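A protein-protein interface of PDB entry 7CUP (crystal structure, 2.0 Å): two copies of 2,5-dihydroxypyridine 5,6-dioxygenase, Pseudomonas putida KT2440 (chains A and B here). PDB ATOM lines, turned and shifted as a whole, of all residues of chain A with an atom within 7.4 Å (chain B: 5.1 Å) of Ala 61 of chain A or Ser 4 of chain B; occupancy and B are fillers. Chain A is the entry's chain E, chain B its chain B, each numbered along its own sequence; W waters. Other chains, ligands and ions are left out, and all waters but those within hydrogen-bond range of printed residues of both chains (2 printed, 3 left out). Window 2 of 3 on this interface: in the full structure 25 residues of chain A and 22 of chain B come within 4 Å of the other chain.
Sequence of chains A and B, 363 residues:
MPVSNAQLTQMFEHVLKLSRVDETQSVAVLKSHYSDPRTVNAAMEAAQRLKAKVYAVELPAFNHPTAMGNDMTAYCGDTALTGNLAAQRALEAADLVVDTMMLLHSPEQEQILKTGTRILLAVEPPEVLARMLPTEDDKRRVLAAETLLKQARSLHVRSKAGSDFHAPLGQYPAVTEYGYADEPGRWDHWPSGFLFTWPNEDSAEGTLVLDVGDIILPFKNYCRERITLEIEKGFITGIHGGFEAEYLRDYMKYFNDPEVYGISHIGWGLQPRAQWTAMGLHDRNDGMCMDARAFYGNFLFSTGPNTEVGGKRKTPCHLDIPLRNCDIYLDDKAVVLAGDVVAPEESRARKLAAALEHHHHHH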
ATOM      1  N   LYS A  31       8.794  31.508  18.232  1.00  0.00           N
ATOM      2  CA  LYS A  31      10.070  30.809  17.911  1.00  0.00           C
ATOM      3  C   LYS A  31       9.842  29.526  17.104  1.00  0.00           C
ATOM      4  O   LYS A  31       8.715  28.992  17.020  1.00  0.00           O
ATOM      5  CB  LYS A  31      10.865  30.488  19.175  1.00  0.00           C
ATOM      6  CG  LYS A  31      10.162  29.552  20.137  1.00  0.00           C
ATOM      7  CD  LYS A  31      10.948  29.282  21.369  1.00  0.00           C
ATOM      8  CE  LYS A  31      10.423  28.073  22.105  1.00  0.00           C
ATOM      9  NZ  LYS A  31      11.247  27.824  23.309  1.00  0.00           N
ATOM     10  N   SER A  32      10.936  29.071  16.516  1.00  0.00           N
ATOM     11  CA  SER A  32      11.059  27.731  15.910  1.00  0.00           C
ATOM     12  C   SER A  32      12.397  27.124  16.354  1.00  0.00           C
ATOM     13  O   SER A  32      13.110  27.786  17.164  1.00  0.00           O
ATOM     14  CB  SER A  32      10.923  27.850  14.420  1.00  0.00           C
ATOM     15  OG  SER A  32      10.538  26.601  13.826  1.00  0.00           O
ATOM     16  N   HIS A  33      12.763  25.951  15.826  1.00  0.00           N
ATOM     17  CA  HIS A  33      13.975  25.204  16.280  1.00  0.00           C
ATOM     18  C   HIS A  33      15.216  26.066  15.999  1.00  0.00           C
ATOM     19  O   HIS A  33      16.193  25.935  16.699  1.00  0.00           O
ATOM     20  CB  HIS A  33      14.081  23.805  15.640  1.00  0.00           C
ATOM     21  CG  HIS A  33      14.512  23.852  14.209  1.00  0.00           C
ATOM     22  ND1 HIS A  33      13.597  23.929  13.157  1.00  0.00           N
ATOM     23  CD2 HIS A  33      15.742  23.882  13.637  1.00  0.00           C
ATOM     24  CE1 HIS A  33      14.271  23.969  12.013  1.00  0.00           C
ATOM     25  NE2 HIS A  33      15.582  23.970  12.285  1.00  0.00           N
ATOM     26  N   TYR A  34      15.172  26.953  15.019  1.00  0.00           N
ATOM     27  CA  TYR A  34      16.374  27.683  14.568  1.00  0.00           C
ATOM     28  C   TYR A  34      16.519  29.034  15.293  1.00  0.00           C
ATOM     29  O   TYR A  34      17.483  29.736  14.998  1.00  0.00           O
ATOM     30  CB  TYR A  34      16.367  27.842  13.047  1.00  0.00           C
ATOM     31  CG  TYR A  34      15.135  28.480  12.471  1.00  0.00           C
ATOM     32  CD1 TYR A  34      14.053  27.707  12.083  1.00  0.00           C
ATOM     33  CD2 TYR A  34      15.036  29.864  12.362  1.00  0.00           C
ATOM     34  CE1 TYR A  34      12.915  28.285  11.550  1.00  0.00           C
ATOM     35  CE2 TYR A  34      13.884  30.456  11.880  1.00  0.00           C
ATOM     36  CZ  TYR A  34      12.835  29.664  11.452  1.00  0.00           C
ATOM     37  OH  TYR A  34      11.705  30.260  10.961  1.00  0.00           O
ATOM     38  N   GLU A  58       5.778  28.035  19.836  1.00  0.00           N
ATOM     39  CA  GLU A  58       6.796  27.365  19.025  1.00  0.00           C
ATOM     40  C   GLU A  58       6.097  26.705  17.840  1.00  0.00           C
ATOM     41  O   GLU A  58       5.149  25.932  18.040  1.00  0.00           O
ATOM     42  CB  GLU A  58       7.621  26.361  19.828  1.00  0.00           C
ATOM     43  CG  GLU A  58       8.624  25.684  18.911  1.00  0.00           C
ATOM     44  CD  GLU A  58       9.778  24.993  19.607  1.00  0.00           C
ATOM     45  OE1 GLU A  58       9.658  24.704  20.851  1.00  0.00           O
ATOM     46  OE2 GLU A  58      10.791  24.754  18.883  1.00  0.00           O
ATOM     47  N   LEU A  59       6.509  27.062  16.638  1.00  0.00           N
ATOM     48  CA  LEU A  59       5.960  26.488  15.390  1.00  0.00           C
ATOM     49  C   LEU A  59       7.017  25.585  14.780  1.00  0.00           C
ATOM     50  O   LEU A  59       8.179  25.961  14.713  1.00  0.00           O
ATOM     51  CB  LEU A  59       5.617  27.602  14.404  1.00  0.00           C
ATOM     52  CG  LEU A  59       4.541  28.576  14.845  1.00  0.00           C
ATOM     53  CD1 LEU A  59       4.304  29.606  13.737  1.00  0.00           C
ATOM     54  CD2 LEU A  59       3.256  27.831  15.174  1.00  0.00           C
ATOM     55  N   PRO A  60       6.612  24.439  14.221  1.00  0.00           N
ATOM     56  CA  PRO A  60       7.519  23.664  13.384  1.00  0.00           C
ATOM     57  C   PRO A  60       8.030  24.559  12.243  1.00  0.00           C
ATOM     58  O   PRO A  60       7.274  25.323  11.694  1.00  0.00           O
ATOM     59  CB  PRO A  60       6.678  22.464  12.885  1.00  0.00           C
ATOM     60  CG  PRO A  60       5.411  22.462  13.766  1.00  0.00           C
ATOM     61  CD  PRO A  60       5.251  23.873  14.310  1.00  0.00           C
ATOM     62  N   ALA A  61       9.314  24.493  11.919  1.00  0.00           N
ATOM     63  CA  ALA A  61       9.884  25.267  10.796  1.00  0.00           C
ATOM     64  C   ALA A  61       9.177  24.915   9.467  1.00  0.00           C
ATOM     65  O   ALA A  61       8.846  23.747   9.217  1.00  0.00           O
ATOM     66  CB  ALA A  61      11.370  25.031  10.722  1.00  0.00           C
ATOM     67  N   PHE A  62       8.987  25.921   8.622  1.00  0.00           N
ATOM     68  CA  PHE A  62       8.436  25.782   7.257  1.00  0.00           C
ATOM     69  C   PHE A  62       9.587  25.797   6.241  1.00  0.00           C
ATOM     70  O   PHE A  62      10.386  26.734   6.279  1.00  0.00           O
ATOM     71  CB  PHE A  62       7.470  26.921   6.917  1.00  0.00           C
ATOM     72  CG  PHE A  62       6.744  26.632   5.635  1.00  0.00           C
ATOM     73  CD1 PHE A  62       5.629  25.812   5.638  1.00  0.00           C
ATOM     74  CD2 PHE A  62       7.242  27.070   4.424  1.00  0.00           C
ATOM     75  CE1 PHE A  62       4.973  25.508   4.455  1.00  0.00           C
ATOM     76  CE2 PHE A  62       6.593  26.758   3.241  1.00  0.00           C
ATOM     77  CZ  PHE A  62       5.464  25.983   3.260  1.00  0.00           C
ATOM     78  N   ASN A  63       9.664  24.793   5.371  1.00  0.00           N
ATOM     79  CA  ASN A  63      10.774  24.725   4.382  1.00  0.00           C
ATOM     80  C   ASN A  63      10.248  25.001   2.963  1.00  0.00           C
ATOM     81  O   ASN A  63       9.228  24.448   2.570  1.00  0.00           O
ATOM     82  CB  ASN A  63      11.585  23.440   4.497  1.00  0.00           C
ATOM     83  CG  ASN A  63      12.897  23.543   3.734  1.00  0.00           C
ATOM     84  OD1 ASN A  63      13.758  24.372   4.092  1.00  0.00           O
ATOM     85  ND2 ASN A  63      13.009  22.776   2.642  1.00  0.00           N
ATOM     86  N   THR A  79       4.492  30.442   4.829  1.00  0.00           N
ATOM     87  CA  THR A  79       5.202  30.434   6.136  1.00  0.00           C
ATOM     88  C   THR A  79       4.609  29.307   6.995  1.00  0.00           C
ATOM     89  O   THR A  79       3.593  28.701   6.594  1.00  0.00           O
ATOM     90  CB  THR A  79       5.087  31.797   6.850  1.00  0.00           C
ATOM     91  OG1 THR A  79       3.747  32.034   7.306  1.00  0.00           O
ATOM     92  CG2 THR A  79       5.528  32.941   5.969  1.00  0.00           C
ATOM     93  N   ALA A  80       5.185  29.090   8.170  1.00  0.00           N
ATOM     94  CA  ALA A  80       4.630  28.208   9.226  1.00  0.00           C
ATOM     95  C   ALA A  80       3.155  28.549   9.527  1.00  0.00           C
ATOM     96  O   ALA A  80       2.419  27.665  10.004  1.00  0.00           O
ATOM     97  CB  ALA A  80       5.525  28.319  10.434  1.00  0.00           C
ATOM     98  N   MET A 101      11.604  34.139  14.664  1.00  0.00           N
ATOM     99  CA  MET A 101      11.632  33.052  13.639  1.00  0.00           C
ATOM    100  C   MET A 101      11.453  33.644  12.243  1.00  0.00           C
ATOM    101  O   MET A 101      11.745  32.979  11.276  1.00  0.00           O
ATOM    102  CB  MET A 101      10.564  31.998  13.930  1.00  0.00           C
ATOM    103  CG  MET A 101       9.180  32.315  13.463  1.00  0.00           C
ATOM    104  SD  MET A 101       8.165  30.826  13.674  1.00  0.00           S
ATOM    105  CE  MET A 101       8.475  29.966  12.131  1.00  0.00           C
ATOM    106  N   PRO B   2      13.316  26.874   6.749  1.00  0.00           N
ATOM    107  CA  PRO B   2      14.193  25.749   7.212  1.00  0.00           C
ATOM    108  C   PRO B   2      13.410  24.450   7.453  1.00  0.00           C
ATOM    109  O   PRO B   2      12.186  24.511   7.494  1.00  0.00           O
ATOM    110  CB  PRO B   2      14.844  26.209   8.529  1.00  0.00           C
ATOM    111  CG  PRO B   2      14.801  27.711   8.429  1.00  0.00           C
ATOM    112  CD  PRO B   2      13.504  27.990   7.697  1.00  0.00           C
ATOM    113  N   VAL B   3      14.129  23.332   7.599  1.00  0.00           N
ATOM    114  CA  VAL B   3      13.558  21.951   7.703  1.00  0.00           C
ATOM    115  C   VAL B   3      13.296  21.602   9.170  1.00  0.00           C
ATOM    116  O   VAL B   3      14.282  21.535   9.938  1.00  0.00           O
ATOM    117  CB  VAL B   3      14.508  20.926   7.063  1.00  0.00           C
ATOM    118  CG1 VAL B   3      14.076  19.492   7.303  1.00  0.00           C
ATOM    119  CG2 VAL B   3      14.652  21.162   5.572  1.00  0.00           C
ATOM    120  N   SER B   4      12.043  21.289   9.514  1.00  0.00           N
ATOM    121  CA  SER B   4      11.594  20.792  10.846  1.00  0.00           C
ATOM    122  C   SER B   4      12.139  19.382  11.110  1.00  0.00           C
ATOM    123  O   SER B   4      12.579  18.725  10.155  1.00  0.00           O
ATOM    124  CB  SER B   4      10.097  20.771  10.978  1.00  0.00           C
ATOM    125  OG  SER B   4       9.545  19.704  10.216  1.00  0.00           O
ATOM    126  N   ASN B   5      12.128  18.942  12.367  1.00  0.00           N
ATOM    127  CA  ASN B   5      12.586  17.579  12.761  1.00  0.00           C
ATOM    128  C   ASN B   5      11.634  16.550  12.141  1.00  0.00           C
ATOM    129  O   ASN B   5      12.127  15.516  11.688  1.00  0.00           O
ATOM    130  CB  ASN B   5      12.665  17.364  14.274  1.00  0.00           C
ATOM    131  CG  ASN B   5      13.798  18.105  14.972  1.00  0.00           C
ATOM    132  OD1 ASN B   5      14.632  18.779  14.366  1.00  0.00           O
ATOM    133  ND2 ASN B   5      13.859  17.958  16.287  1.00  0.00           N
ATOM    134  N   ALA B   6      10.331  16.823  12.132  1.00  0.00           N
ATOM    135  CA  ALA B   6       9.308  15.945  11.511  1.00  0.00           C
ATOM    136  C   ALA B   6       9.639  15.766  10.027  1.00  0.00           C
ATOM    137  O   ALA B   6       9.661  14.621   9.547  1.00  0.00           O
ATOM    138  CB  ALA B   6       7.914  16.517  11.672  1.00  0.00           C
ATOM    139  N   GLN B   7       9.858  16.855   9.310  1.00  0.00           N
ATOM    140  CA  GLN B   7      10.138  16.783   7.865  1.00  0.00           C
ATOM    141  C   GLN B   7      11.481  16.079   7.633  1.00  0.00           C
ATOM    142  O   GLN B   7      11.546  15.303   6.673  1.00  0.00           O
ATOM    143  CB  GLN B   7      10.080  18.157   7.208  1.00  0.00           C
ATOM    144  CG  GLN B   7      10.581  18.125   5.774  1.00  0.00           C
ATOM    145  CD  GLN B   7      10.277  19.365   4.977  1.00  0.00           C
ATOM    146  OE1 GLN B   7       9.288  20.045   5.213  1.00  0.00           O
ATOM    147  NE2 GLN B   7      11.106  19.635   3.985  1.00  0.00           N
ATOM    148  N   LEU B   8      12.508  16.338   8.444  1.00  0.00           N
ATOM    149  CA  LEU B   8      13.807  15.638   8.279  1.00  0.00           C
ATOM    150  C   LEU B   8      13.639  14.113   8.447  1.00  0.00           C
ATOM    151  O   LEU B   8      14.214  13.369   7.638  1.00  0.00           O
ATOM    152  CB  LEU B   8      14.809  16.204   9.274  1.00  0.00           C
ATOM    153  CG  LEU B   8      16.261  15.807   9.083  1.00  0.00           C
ATOM    154  CD1 LEU B   8      16.742  16.069   7.673  1.00  0.00           C
ATOM    155  CD2 LEU B   8      17.119  16.553  10.087  1.00  0.00           C
ATOM    156  N   ARG B  38      20.629  16.447  14.831  1.00  0.00           N
ATOM    157  CA  ARG B  38      19.279  16.373  14.214  1.00  0.00           C
ATOM    158  C   ARG B  38      19.241  15.331  13.078  1.00  0.00           C
ATOM    159  O   ARG B  38      18.265  14.620  12.981  1.00  0.00           O
ATOM    160  CB  ARG B  38      18.896  17.762  13.722  1.00  0.00           C
ATOM    161  CG  ARG B  38      18.808  18.751  14.869  1.00  0.00           C
ATOM    162  CD  ARG B  38      18.502  20.116  14.315  1.00  0.00           C
ATOM    163  NE  ARG B  38      17.139  20.059  13.823  1.00  0.00           N
ATOM    164  CZ  ARG B  38      16.739  20.418  12.612  1.00  0.00           C
ATOM    165  NH1 ARG B  38      17.611  20.887  11.733  1.00  0.00           N
ATOM    166  NH2 ARG B  38      15.451  20.311  12.307  1.00  0.00           N
HETATM  167  O   HOH W   1      11.192  21.005   1.887  1.00  0.00           O
HETATM  168  O   HOH W   2       7.678  22.739   5.461  1.00  0.00           O
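Water W1 bridges the side-chain amide nitrogen (NE2) of Gln 7 of chain B (2.5 Å) and the side-chain amide nitrogen (ND2) of Asn 63 of chain A (2.6 Å). Water W2 lies within hydrogen-bond range of the backbone NH (N) of Asn 63 of chain A (2.9 Å) and the side-chain amide oxygen (OE1) of Gln 7 of chain B (3.1 Å).
Of the 13 printed residues of chain A, 5 touch a printed residue of chain B. Hydrophobic or aromatic side chains of chain A that line the printed part of chain B: His 33, Tyr 34 and Ala 61. Printed residues of chain B that touch a printed residue of chain A: Pro 2, Val 3, Ser 4, Gln 7 and Arg 38. Among the printed residues, 9 pairs touch across the chains. Among the printed residues, no Asp or Glu carboxylate lies within 4 Å of a Lys or Arg side-chain nitrogen of the other chain.
Ala 61 of chain A touches two residues of chain B. Of the printed residues of chain A, Ser 4 of chain B touches Ala 61 (3.7 Å). Of the printed residues of chain A, Gln 7 of chain B touches Asn 63 (3.9 Å). Of the printed residues of chain B, Tyr 34 of chain A touches Pro 2 (3.7 Å). Printed residues of chain B within 4 Å of Phe 62 of chain A: Pro 2. Of the printed residues of chain A, Val 3 of chain B touches His 33 and Asn 63. Printed residues of chain B within 4 Å of His 33 of chain A: Val 3 (3.2 Å) and Arg 38 (3.7 Å). The nearest residue of chain B that does not touch Ala 61 of chain A is Val 3 of chain B (4.2 Å). The nearest printed residue of chain A that does not touch Ser 4 of chain B is Pro 60 of chain A (4.3 Å). The nearest printed residue of chain A that does not touch Arg 38 of chain B is Ala 61 of chain A (6.4 Å).
No position is printed for both chains.
The guanidinium group (NH2) of Arg 38 of chain B sits at hydrogen-bond distance from the backbone carbonyl oxygen (O) of Val 3 of chain B (2.9 Å). The backbone NH (N) of Gln 7 of chain B sits at hydrogen-bond distance from the side-chain hydroxyl (OG) of Ser 4 of chain B, 3.0 Å away. NH2 of Arg 38 of chain B lies within hydrogen-bond range of OD1 of Asn 5 of chain B (2.7 Å). N of Ala 61 of chain A lies within hydrogen-bond range of OG of Ser 32 of chain A. OH of Tyr 34 of chain A is in hydrogen-bond range of O of Met 101 of chain A, 2.7 Å away.
The backbone carbonyl oxygen of Pro 2 of chain B sits close to the backbone NH of Asn 63 of chain A, at 3.3 Å. The backbone nitrogen (N) of Pro 2 of chain B lies close to the backbone carbonyl oxygen (O) of Phe 62 of chain A (3.0 Å).
Among the printed residues, pairs that only touch across the chains: His 33 of chain A with Val 3 of chain B (3.2 Å), His 33 of chain A with Arg 38 of chain B (3.7 Å), Tyr 34 of chain A with Pro 2 of chain B (3.7 Å), Ala 61 of chain A with Pro 2 of chain B (3.4 Å), Ala 61 of chain A with Ser 4 of chain B (3.7 Å), Asn 63 of chain A with Val 3 of chain B (3.5 Å) and Asn 63 of chain A with Gln 7 of chain B (3.9 Å).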
